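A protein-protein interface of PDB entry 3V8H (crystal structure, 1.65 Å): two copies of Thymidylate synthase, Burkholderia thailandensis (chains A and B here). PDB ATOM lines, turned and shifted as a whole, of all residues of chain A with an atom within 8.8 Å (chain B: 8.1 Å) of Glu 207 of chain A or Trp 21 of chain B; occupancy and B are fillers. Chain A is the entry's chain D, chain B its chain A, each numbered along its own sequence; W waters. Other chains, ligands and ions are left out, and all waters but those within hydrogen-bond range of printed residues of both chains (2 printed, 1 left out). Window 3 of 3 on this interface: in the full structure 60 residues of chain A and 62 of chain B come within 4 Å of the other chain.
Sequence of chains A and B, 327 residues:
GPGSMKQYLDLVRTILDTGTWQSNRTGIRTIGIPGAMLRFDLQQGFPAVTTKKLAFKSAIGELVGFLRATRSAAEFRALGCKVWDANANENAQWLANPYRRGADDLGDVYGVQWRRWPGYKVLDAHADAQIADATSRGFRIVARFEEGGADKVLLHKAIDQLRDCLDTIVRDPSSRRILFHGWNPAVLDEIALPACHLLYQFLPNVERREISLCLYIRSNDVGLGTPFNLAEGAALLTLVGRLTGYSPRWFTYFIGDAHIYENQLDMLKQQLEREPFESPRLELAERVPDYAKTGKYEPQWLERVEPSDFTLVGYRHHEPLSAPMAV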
ATOM      1  N   PRO A 173      10.405 -25.843  -3.854  1.00  0.00           N
ATOM      2  CA  PRO A 173      11.616 -25.023  -3.944  1.00  0.00           C
ATOM      3  C   PRO A 173      12.591 -25.078  -2.779  1.00  0.00           C
ATOM      4  O   PRO A 173      13.734 -24.623  -2.949  1.00  0.00           O
ATOM      5  CB  PRO A 173      11.058 -23.608  -4.064  1.00  0.00           C
ATOM      6  CG  PRO A 173       9.732 -23.675  -3.372  1.00  0.00           C
ATOM      7  CD  PRO A 173       9.194 -25.015  -3.746  1.00  0.00           C
ATOM      8  N   SER A 174      12.179 -25.612  -1.618  1.00  0.00           N
ATOM      9  CA  SER A 174      13.122 -25.797  -0.506  1.00  0.00           C
ATOM     10  C   SER A 174      14.026 -26.995  -0.689  1.00  0.00           C
ATOM     11  O   SER A 174      14.948 -27.168   0.112  1.00  0.00           O
ATOM     12  CB  SER A 174      12.428 -25.859   0.856  1.00  0.00           C
ATOM     13  OG  SER A 174      11.785 -27.086   1.061  1.00  0.00           O
ATOM     14  N   PRO A 204      16.632 -21.847  -5.235  1.00  0.00           N
ATOM     15  CA  PRO A 204      15.521 -20.935  -5.004  1.00  0.00           C
ATOM     16  C   PRO A 204      15.390 -20.532  -3.559  1.00  0.00           C
ATOM     17  O   PRO A 204      15.603 -21.352  -2.658  1.00  0.00           O
ATOM     18  CB  PRO A 204      14.289 -21.719  -5.463  1.00  0.00           C
ATOM     19  CG  PRO A 204      14.753 -23.103  -5.782  1.00  0.00           C
ATOM     20  CD  PRO A 204      16.215 -23.230  -5.514  1.00  0.00           C
ATOM     21  N   ASN A 205      15.053 -19.263  -3.347  1.00  0.00           N
ATOM     22  CA  ASN A 205      14.812 -18.699  -2.031  1.00  0.00           C
ATOM     23  C   ASN A 205      13.370 -18.232  -2.077  1.00  0.00           C
ATOM     24  O   ASN A 205      13.059 -17.218  -2.680  1.00  0.00           O
ATOM     25  CB  ASN A 205      15.800 -17.552  -1.773  1.00  0.00           C
ATOM     26  CG  ASN A 205      15.612 -16.891  -0.412  1.00  0.00           C
ATOM     27  OD1 ASN A 205      14.511 -16.795   0.065  1.00  0.00           O
ATOM     28  ND2 ASN A 205      16.696 -16.395   0.181  1.00  0.00           N
ATOM     29  N   VAL A 206      12.474 -19.012  -1.479  1.00  0.00           N
ATOM     30  CA  VAL A 206      11.034 -18.791  -1.698  1.00  0.00           C
ATOM     31  C   VAL A 206      10.578 -17.540  -0.938  1.00  0.00           C
ATOM     32  O   VAL A 206       9.720 -16.807  -1.440  1.00  0.00           O
ATOM     33  CB  VAL A 206      10.179 -20.088  -1.481  1.00  0.00           C
ATOM     34  CG1 VAL A 206      10.036 -20.400  -0.022  1.00  0.00           C
ATOM     35  CG2 VAL A 206       8.792 -19.966  -2.125  1.00  0.00           C
ATOM     36  N   GLU A 207      11.198 -17.243   0.204  1.00  0.00           N
ATOM     37  CA  GLU A 207      10.860 -16.036   0.994  1.00  0.00           C
ATOM     38  C   GLU A 207      11.161 -14.714   0.218  1.00  0.00           C
ATOM     39  O   GLU A 207      10.462 -13.722   0.346  1.00  0.00           O
ATOM     40  CB  GLU A 207      11.548 -16.074   2.376  1.00  0.00           C
ATOM     41  CG  GLU A 207      11.063 -17.184   3.322  1.00  0.00           C
ATOM     42  CD  GLU A 207      11.583 -18.593   3.020  1.00  0.00           C
ATOM     43  OE1 GLU A 207      12.479 -18.750   2.144  1.00  0.00           O
ATOM     44  OE2 GLU A 207      11.074 -19.572   3.661  1.00  0.00           O
ATOM     45  N   ARG A 208      12.159 -14.730  -0.660  1.00  0.00           N
ATOM     46  CA  ARG A 208      12.535 -13.542  -1.416  1.00  0.00           C
ATOM     47  C   ARG A 208      12.201 -13.672  -2.910  1.00  0.00           C
ATOM     48  O   ARG A 208      12.377 -12.722  -3.659  1.00  0.00           O
ATOM     49  CB  ARG A 208      14.027 -13.297  -1.240  1.00  0.00           C
ATOM     50  CG  ARG A 208      14.421 -13.260   0.238  1.00  0.00           C
ATOM     51  CD  ARG A 208      15.900 -13.102   0.398  1.00  0.00           C
ATOM     52  NE  ARG A 208      16.284 -11.709   0.409  1.00  0.00           N
ATOM     53  CZ  ARG A 208      15.986 -10.837   1.379  1.00  0.00           C
ATOM     54  NH1 ARG A 208      15.253 -11.166   2.457  1.00  0.00           N
ATOM     55  NH2 ARG A 208      16.408  -9.601   1.245  1.00  0.00           N
ATOM     56  N   ARG A 209      11.707 -14.831  -3.320  1.00  0.00           N
ATOM     57  CA  ARG A 209      11.507 -15.214  -4.729  1.00  0.00           C
ATOM     58  C   ARG A 209      12.696 -14.849  -5.605  1.00  0.00           C
ATOM     59  O   ARG A 209      12.557 -14.292  -6.725  1.00  0.00           O
ATOM     60  CB  ARG A 209      10.183 -14.637  -5.266  1.00  0.00           C
ATOM     61  CG  ARG A 209       8.960 -15.125  -4.510  1.00  0.00           C
ATOM     62  CD  ARG A 209       8.779 -16.637  -4.581  1.00  0.00           C
ATOM     63  NE  ARG A 209       8.368 -17.006  -5.901  1.00  0.00           N
ATOM     64  CZ  ARG A 209       7.110 -17.160  -6.322  1.00  0.00           C
ATOM     65  NH1 ARG A 209       6.069 -17.025  -5.500  1.00  0.00           N
ATOM     66  NH2 ARG A 209       6.893 -17.434  -7.596  1.00  0.00           N
ATOM     67  N   GLU A 210      13.873 -15.144  -5.046  1.00  0.00           N
ATOM     68  CA  GLU A 210      15.163 -15.040  -5.741  1.00  0.00           C
ATOM     69  C   GLU A 210      15.726 -16.415  -6.062  1.00  0.00           C
ATOM     70  O   GLU A 210      15.616 -17.308  -5.258  1.00  0.00           O
ATOM     71  CB  GLU A 210      16.140 -14.244  -4.873  1.00  0.00           C
ATOM     72  CG  GLU A 210      15.743 -12.782  -4.701  1.00  0.00           C
ATOM     73  CD  GLU A 210      16.666 -11.994  -3.779  1.00  0.00           C
ATOM     74  OE1 GLU A 210      17.652 -12.549  -3.256  1.00  0.00           O
ATOM     75  OE2 GLU A 210      16.399 -10.798  -3.557  1.00  0.00           O
ATOM     76  N   TYR A 246      10.865 -16.773 -10.328  1.00  0.00           N
ATOM     77  CA  TYR A 246      11.950 -16.286  -9.465  1.00  0.00           C
ATOM     78  C   TYR A 246      12.833 -15.302 -10.190  1.00  0.00           C
ATOM     79  O   TYR A 246      13.096 -15.462 -11.397  1.00  0.00           O
ATOM     80  CB  TYR A 246      12.841 -17.447  -8.970  1.00  0.00           C
ATOM     81  CG  TYR A 246      12.191 -18.316  -7.963  1.00  0.00           C
ATOM     82  CD1 TYR A 246      11.262 -19.289  -8.347  1.00  0.00           C
ATOM     83  CD2 TYR A 246      12.391 -18.125  -6.602  1.00  0.00           C
ATOM     84  CE1 TYR A 246      10.611 -20.042  -7.399  1.00  0.00           C
ATOM     85  CE2 TYR A 246      11.779 -18.898  -5.668  1.00  0.00           C
ATOM     86  CZ  TYR A 246      10.827 -19.811  -6.051  1.00  0.00           C
ATOM     87  OH  TYR A 246      10.167 -20.591  -5.120  1.00  0.00           O
ATOM     88  N   ILE B  15      27.525 -16.188   6.852  1.00  0.00           N
ATOM     89  CA  ILE B  15      26.173 -16.744   6.743  1.00  0.00           C
ATOM     90  C   ILE B  15      25.245 -16.064   7.759  1.00  0.00           C
ATOM     91  O   ILE B  15      24.146 -15.637   7.404  1.00  0.00           O
ATOM     92  CB  ILE B  15      26.178 -18.270   6.934  1.00  0.00           C
ATOM     93  CG1 ILE B  15      26.931 -18.948   5.780  1.00  0.00           C
ATOM     94  CG2 ILE B  15      24.764 -18.824   7.001  1.00  0.00           C
ATOM     95  CD1 ILE B  15      27.152 -20.431   5.982  1.00  0.00           C
ATOM     96  N   LEU B  16      25.707 -15.935   9.003  1.00  0.00           N
ATOM     97  CA  LEU B  16      24.899 -15.285  10.046  1.00  0.00           C
ATOM     98  C   LEU B  16      24.652 -13.805   9.753  1.00  0.00           C
ATOM     99  O   LEU B  16      23.590 -13.293  10.061  1.00  0.00           O
ATOM    100  CB  LEU B  16      25.538 -15.465  11.426  1.00  0.00           C
ATOM    101  CG  LEU B  16      25.689 -16.896  11.940  1.00  0.00           C
ATOM    102  CD1 LEU B  16      26.401 -16.938  13.287  1.00  0.00           C
ATOM    103  CD2 LEU B  16      24.343 -17.612  12.020  1.00  0.00           C
ATOM    104  N   THR B  18      24.881 -12.227   6.568  1.00  0.00           N
ATOM    105  CA  THR B  18      24.360 -11.929   5.218  1.00  0.00           C
ATOM    106  C   THR B  18      23.319 -12.942   4.689  1.00  0.00           C
ATOM    107  O   THR B  18      22.680 -12.696   3.670  1.00  0.00           O
ATOM    108  CB  THR B  18      25.506 -11.835   4.185  1.00  0.00           C
ATOM    109  OG1 THR B  18      26.057 -13.141   3.953  1.00  0.00           O
ATOM    110  CG2 THR B  18      26.619 -10.888   4.674  1.00  0.00           C
ATOM    111  N   GLY B  19      23.146 -14.063   5.384  1.00  0.00           N
ATOM    112  CA  GLY B  19      22.193 -15.087   4.982  1.00  0.00           C
ATOM    113  C   GLY B  19      20.754 -14.682   5.197  1.00  0.00           C
ATOM    114  O   GLY B  19      20.459 -13.686   5.838  1.00  0.00           O
ATOM    115  N   THR B  20      19.851 -15.482   4.651  1.00  0.00           N
ATOM    116  CA  THR B  20      18.418 -15.255   4.784  1.00  0.00           C
ATOM    117  C   THR B  20      17.757 -16.532   5.363  1.00  0.00           C
ATOM    118  O   THR B  20      18.282 -17.645   5.189  1.00  0.00           O
ATOM    119  CB  THR B  20      17.844 -14.853   3.403  1.00  0.00           C
ATOM    120  OG1 THR B  20      18.135 -15.882   2.447  1.00  0.00           O
ATOM    121  CG2 THR B  20      18.497 -13.568   2.912  1.00  0.00           C
ATOM    122  N   TRP B  21      16.655 -16.366   6.085  1.00  0.00           N
ATOM    123  CA  TRP B  21      15.974 -17.482   6.770  1.00  0.00           C
ATOM    124  C   TRP B  21      15.010 -18.213   5.879  1.00  0.00           C
ATOM    125  O   TRP B  21      14.215 -17.576   5.157  1.00  0.00           O
ATOM    126  CB  TRP B  21      15.231 -16.991   8.014  1.00  0.00           C
ATOM    127  CG  TRP B  21      16.163 -16.716   9.160  1.00  0.00           C
ATOM    128  CD1 TRP B  21      16.566 -15.483   9.644  1.00  0.00           C
ATOM    129  CD2 TRP B  21      16.864 -17.704   9.988  1.00  0.00           C
ATOM    130  NE1 TRP B  21      17.433 -15.633  10.696  1.00  0.00           N
ATOM    131  CE2 TRP B  21      17.668 -16.942  10.938  1.00  0.00           C
ATOM    132  CE3 TRP B  21      16.925 -19.092  10.011  1.00  0.00           C
ATOM    133  CZ2 TRP B  21      18.477 -17.558  11.872  1.00  0.00           C
ATOM    134  CZ3 TRP B  21      17.741 -19.707  10.963  1.00  0.00           C
ATOM    135  CH2 TRP B  21      18.506 -18.952  11.864  1.00  0.00           C
ATOM    136  N   GLN B  22      15.060 -19.550   5.933  1.00  0.00           N
ATOM    137  CA  GLN B  22      14.182 -20.430   5.141  1.00  0.00           C
ATOM    138  C   GLN B  22      13.635 -21.636   5.896  1.00  0.00           C
ATOM    139  O   GLN B  22      14.328 -22.215   6.731  1.00  0.00           O
ATOM    140  CB  GLN B  22      14.926 -20.950   3.911  1.00  0.00           C
ATOM    141  CG  GLN B  22      15.434 -19.843   3.017  1.00  0.00           C
ATOM    142  CD  GLN B  22      15.522 -20.256   1.568  1.00  0.00           C
ATOM    143  OE1 GLN B  22      14.483 -20.448   0.889  1.00  0.00           O
ATOM    144  NE2 GLN B  22      16.754 -20.362   1.065  1.00  0.00           N
ATOM    145  N   SER B  23      12.404 -22.027   5.560  1.00  0.00           N
ATOM    146  CA  SER B  23      11.772 -23.252   6.074  1.00  0.00           C
ATOM    147  C   SER B  23      11.912 -24.414   5.073  1.00  0.00           C
ATOM    148  O   SER B  23      12.028 -24.186   3.865  1.00  0.00           O
ATOM    149  CB  SER B  23      10.307 -22.973   6.357  1.00  0.00           C
ATOM    150  OG  SER B  23      10.188 -21.791   7.133  1.00  0.00           O
ATOM    151  N   ASN B  24      11.907 -25.651   5.572  1.00  0.00           N
ATOM    152  CA  ASN B  24      12.194 -26.839   4.744  1.00  0.00           C
ATOM    153  C   ASN B  24      11.370 -28.075   5.129  1.00  0.00           C
ATOM    154  O   ASN B  24      11.033 -28.270   6.297  1.00  0.00           O
ATOM    155  CB  ASN B  24      13.691 -27.168   4.802  1.00  0.00           C
ATOM    156  CG  ASN B  24      14.240 -27.162   6.223  1.00  0.00           C
ATOM    157  OD1 ASN B  24      14.042 -28.119   6.976  1.00  0.00           O
ATOM    158  ND2 ASN B  24      14.925 -26.077   6.598  1.00  0.00           N
ATOM    159  N   ILE B  28      12.975 -27.620  10.987  1.00  0.00           N
ATOM    160  CA  ILE B  28      13.902 -26.658  11.591  1.00  0.00           C
ATOM    161  C   ILE B  28      14.351 -25.684  10.504  1.00  0.00           C
ATOM    162  O   ILE B  28      14.852 -26.106   9.453  1.00  0.00           O
ATOM    163  CB  ILE B  28      15.149 -27.359  12.197  1.00  0.00           C
ATOM    164  CG1 ILE B  28      14.757 -28.446  13.226  1.00  0.00           C
ATOM    165  CG2 ILE B  28      16.112 -26.337  12.808  1.00  0.00           C
ATOM    166  CD1 ILE B  28      14.434 -27.943  14.627  1.00  0.00           C
ATOM    167  N   ARG B  29      14.193 -24.392  10.766  1.00  0.00           N
ATOM    168  CA  ARG B  29      14.596 -23.363   9.819  1.00  0.00           C
ATOM    169  C   ARG B  29      16.114 -23.334   9.636  1.00  0.00           C
ATOM    170  O   ARG B  29      16.864 -23.698  10.544  1.00  0.00           O
ATOM    171  CB  ARG B  29      14.179 -21.979  10.296  1.00  0.00           C
ATOM    172  CG  ARG B  29      12.681 -21.740  10.339  1.00  0.00           C
ATOM    173  CD  ARG B  29      12.381 -20.255  10.315  1.00  0.00           C
ATOM    174  NE  ARG B  29      13.104 -19.527  11.355  1.00  0.00           N
ATOM    175  CZ  ARG B  29      13.227 -18.201  11.410  1.00  0.00           C
ATOM    176  NH1 ARG B  29      13.919 -17.642  12.397  1.00  0.00           N
ATOM    177  NH2 ARG B  29      12.669 -17.424  10.493  1.00  0.00           N
ATOM    178  N   THR B  30      16.537 -22.826   8.476  1.00  0.00           N
ATOM    179  CA  THR B  30      17.956 -22.641   8.208  1.00  0.00           C
ATOM    180  C   THR B  30      18.239 -21.220   7.734  1.00  0.00           C
ATOM    181  O   THR B  30      17.373 -20.564   7.139  1.00  0.00           O
ATOM    182  CB  THR B  30      18.457 -23.650   7.150  1.00  0.00           C
ATOM    183  OG1 THR B  30      17.713 -23.449   5.943  1.00  0.00           O
ATOM    184  CG2 THR B  30      18.265 -25.074   7.629  1.00  0.00           C
ATOM    185  N   ILE B  31      19.453 -20.746   8.013  1.00  0.00           N
ATOM    186  CA  ILE B  31      19.973 -19.505   7.446  1.00  0.00           C
ATOM    187  C   ILE B  31      21.124 -19.903   6.497  1.00  0.00           C
ATOM    188  O   ILE B  31      21.924 -20.734   6.834  1.00  0.00           O
ATOM    189  CB  ILE B  31      20.399 -18.503   8.539  1.00  0.00           C
ATOM    190  CG1 ILE B  31      20.868 -17.178   7.905  1.00  0.00           C
ATOM    191  CG2 ILE B  31      21.414 -19.104   9.511  1.00  0.00           C
ATOM    192  CD1 ILE B  31      20.749 -15.979   8.835  1.00  0.00           C
ATOM    193  N   GLY B  32      21.157 -19.358   5.289  1.00  0.00           N
ATOM    194  CA  GLY B  32      22.078 -19.852   4.272  1.00  0.00           C
ATOM    195  C   GLY B  32      22.480 -18.829   3.236  1.00  0.00           C
ATOM    196  O   GLY B  32      21.853 -17.764   3.115  1.00  0.00           O
ATOM    197  N   ILE B 260      23.060 -23.022   7.942  1.00  0.00           N
ATOM    198  CA  ILE B 260      23.156 -23.296   9.355  1.00  0.00           C
ATOM    199  C   ILE B 260      21.740 -23.470   9.884  1.00  0.00           C
ATOM    200  O   ILE B 260      20.829 -22.703   9.540  1.00  0.00           O
ATOM    201  CB  ILE B 260      23.840 -22.126  10.067  1.00  0.00           C
ATOM    202  CG1 ILE B 260      25.321 -22.112   9.699  1.00  0.00           C
ATOM    203  CG2 ILE B 260      23.633 -22.219  11.588  1.00  0.00           C
ATOM    204  CD1 ILE B 260      26.019 -20.847  10.130  1.00  0.00           C
ATOM    205  N   TYR B 261      21.572 -24.485  10.725  1.00  0.00           N
ATOM    206  CA  TYR B 261      20.278 -24.781  11.348  1.00  0.00           C
ATOM    207  C   TYR B 261      20.045 -23.889  12.572  1.00  0.00           C
ATOM    208  O   TYR B 261      20.974 -23.588  13.333  1.00  0.00           O
ATOM    209  CB  TYR B 261      20.225 -26.252  11.745  1.00  0.00           C
ATOM    210  CG  TYR B 261      19.980 -27.175  10.597  1.00  0.00           C
ATOM    211  CD1 TYR B 261      18.693 -27.511  10.209  1.00  0.00           C
ATOM    212  CD2 TYR B 261      21.031 -27.706   9.889  1.00  0.00           C
ATOM    213  CE1 TYR B 261      18.467 -28.364   9.141  1.00  0.00           C
ATOM    214  CE2 TYR B 261      20.820 -28.549   8.825  1.00  0.00           C
ATOM    215  CZ  TYR B 261      19.535 -28.874   8.450  1.00  0.00           C
ATOM    216  OH  TYR B 261      19.314 -29.723   7.390  1.00  0.00           O
ATOM    217  N   GLU B 262      18.798 -23.466  12.749  1.00  0.00           N
ATOM    218  CA  GLU B 262      18.449 -22.502  13.798  1.00  0.00           C
ATOM    219  C   GLU B 262      18.764 -23.075  15.173  1.00  0.00           C
ATOM    220  O   GLU B 262      19.219 -22.329  16.034  1.00  0.00           O
ATOM    221  CB  GLU B 262      16.972 -22.074  13.738  1.00  0.00           C
ATOM    222  CG  GLU B 262      16.646 -20.960  14.715  1.00  0.00           C
ATOM    223  CD  GLU B 262      15.445 -20.120  14.318  1.00  0.00           C
ATOM    224  OE1 GLU B 262      14.511 -20.666  13.694  1.00  0.00           O
ATOM    225  OE2 GLU B 262      15.441 -18.905  14.640  1.00  0.00           O
ATOM    226  N   ASN B 263      18.553 -24.383  15.355  1.00  0.00           N
ATOM    227  CA  ASN B 263      18.785 -25.036  16.663  1.00  0.00           C
ATOM    228  C   ASN B 263      20.268 -25.282  16.971  1.00  0.00           C
ATOM    229  O   ASN B 263      20.606 -25.858  18.002  1.00  0.00           O
ATOM    230  CB  ASN B 263      17.962 -26.339  16.844  1.00  0.00           C
ATOM    231  CG  ASN B 263      18.282 -27.420  15.808  1.00  0.00           C
ATOM    232  OD1 ASN B 263      19.123 -27.234  14.921  1.00  0.00           O
ATOM    233  ND2 ASN B 263      17.583 -28.558  15.903  1.00  0.00           N
ATOM    234  N   GLN B 264      21.155 -24.824  16.087  1.00  0.00           N
ATOM    235  CA  GLN B 264      22.592 -24.863  16.329  1.00  0.00           C
ATOM    236  C   GLN B 264      23.198 -23.496  16.664  1.00  0.00           C
ATOM    237  O   GLN B 264      24.380 -23.415  16.986  1.00  0.00           O
ATOM    238  CB  GLN B 264      23.311 -25.467  15.109  1.00  0.00           C
ATOM    239  CG  GLN B 264      23.196 -26.981  15.034  1.00  0.00           C
ATOM    240  CD  GLN B 264      23.827 -27.565  13.782  1.00  0.00           C
ATOM    241  OE1 GLN B 264      24.987 -27.288  13.490  1.00  0.00           O
ATOM    242  NE2 GLN B 264      23.093 -28.421  13.083  1.00  0.00           N
ATOM    243  N   LEU B 265      22.409 -22.425  16.583  1.00  0.00           N
ATOM    244  CA  LEU B 265      22.938 -21.057  16.703  1.00  0.00           C
ATOM    245  C   LEU B 265      23.724 -20.778  17.980  1.00  0.00           C
ATOM    246  O   LEU B 265      24.787 -20.142  17.940  1.00  0.00           O
ATOM    247  CB  LEU B 265      21.796 -20.037  16.632  1.00  0.00           C
ATOM    248  CG  LEU B 265      21.273 -19.681  15.254  1.00  0.00           C
ATOM    249  CD1 LEU B 265      20.055 -18.776  15.393  1.00  0.00           C
ATOM    250  CD2 LEU B 265      22.380 -19.017  14.446  1.00  0.00           C
HETATM  251  O   HOH W   1      18.103 -21.306  -1.345  1.00  0.00           O
HETATM  252  O   HOH W   2      15.077 -16.117   2.826  1.00  0.00           O
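The side-chain hydroxyl of Thr 20 of chain B is in hydrogen-bond range of the side-chain amide nitrogen of Asn 205 of chain A. The side-chain amide oxygen of Gln 22 of chain B lies within hydrogen-bond range of the backbone NH of Val 206 of chain A, at 3.4 Å. The side-chain amide oxygen (OE1) of Gln 22 of chain B sits close to the side-chain carboxylate (OE1) of Glu 207 of chain A, 2.9 Å away. The backbone NH of Ser 23 of chain B is in hydrogen-bond range of the side-chain carboxylate of Glu 207 of chain A (3.4 Å).
The backbone NH of Gly 32 of chain B lies within hydrogen-bond range of the backbone carbonyl oxygen of Thr 20 of chain B (3.3 Å). N of Gln 22 of chain B is in hydrogen-bond range of O of Thr 30 of chain B, at 2.8 Å. ND2 of Asn 24 of chain B lies within hydrogen-bond range of O of Ile 28 of chain B, 2.9 Å away. OD1 of Asn 205 of chain A lies close to N of Glu 207 of chain A (3.3 Å). The side-chain amide oxygen of Asn 205 of chain A lies within hydrogen-bond range of the backbone NH of Arg 208 of chain A (3.2 Å). The backbone carbonyl oxygen of Glu 210 of chain A sits at hydrogen-bond distance from the backbone NH of Asn 205 of chain A, 2.8 Å away.
Printed residues of chain B within 4 Å of Glu 207 of chain A: Trp 21, Gln 22 and Ser 23. Of chain A, only Glu 207 (3.5 Å) comes within 4 Å of Trp 21 of chain B. Gln 22 of chain B touches four residues of chain A. Of the printed residues of chain B, Pro 204 of chain A touches Gln 22. Printed residues of chain B within 4 Å of Ser 174 of chain A: Ser 23 and Asn 24. Of the printed residues of chain A, Asn 24 of chain B touches Ser 174 (3.7 Å). Of the printed residues of chain A, Ser 23 of chain B touches Ser 174 (3.5 Å) and Glu 207 (3.4 Å). Asn 263 of chain B touches none of the printed residues of chain A. The nearest printed residue of chain B that does not touch Pro 204 of chain A is Thr 20 of chain B (7.9 Å).
No position is printed for both chains. Of the 10 pairs that touch across the chains among the printed residues, none has its exchanged pair printed and touching as well.
Ser 174 of chain A touches Ser 23 of chain B. OG of Ser 174 of chain A touches CA of Asn 24 of chain B, at 3.7 Å. Pro 204 of chain A touches Gln 22 of chain B (O to OE1, 3.8 Å). OE1 of Gln 22 of chain B touches CA of Asn 205 of chain A, at 3.4 Å. Glu 207 of chain A touches Trp 21 of chain B (CD to O, 3.5 Å). Thr 20 of chain B touches Arg 208 of chain A.
Of the 20 printed residues of chain B, 5 touch a printed residue of chain A. Printed residues of chain B that touch a printed residue of chain A: Thr 20, Trp 21, Gln 22, Ser 23 and Asn 24. Among the printed residues, 10 pairs touch across the chains. Among the printed residues, no Asp or Glu carboxylate lies within 4 Å of a Lys or Arg side-chain nitrogen of the other chain.
Water W1 lies within hydrogen-bond range of the backbone carbonyl oxygen (O) of Pro 204 of chain A and the side-chain amide nitrogen (NE2) of Gln 22 of chain B. Water W2 lies within hydrogen-bond range of the backbone carbonyl oxygen (O) of Trp 21 of chain B, the side-chain amide oxygen (OD1) of Asn 205 of chain A and the side-chain hydroxyl (OG1) of Thr 20 of chain B.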
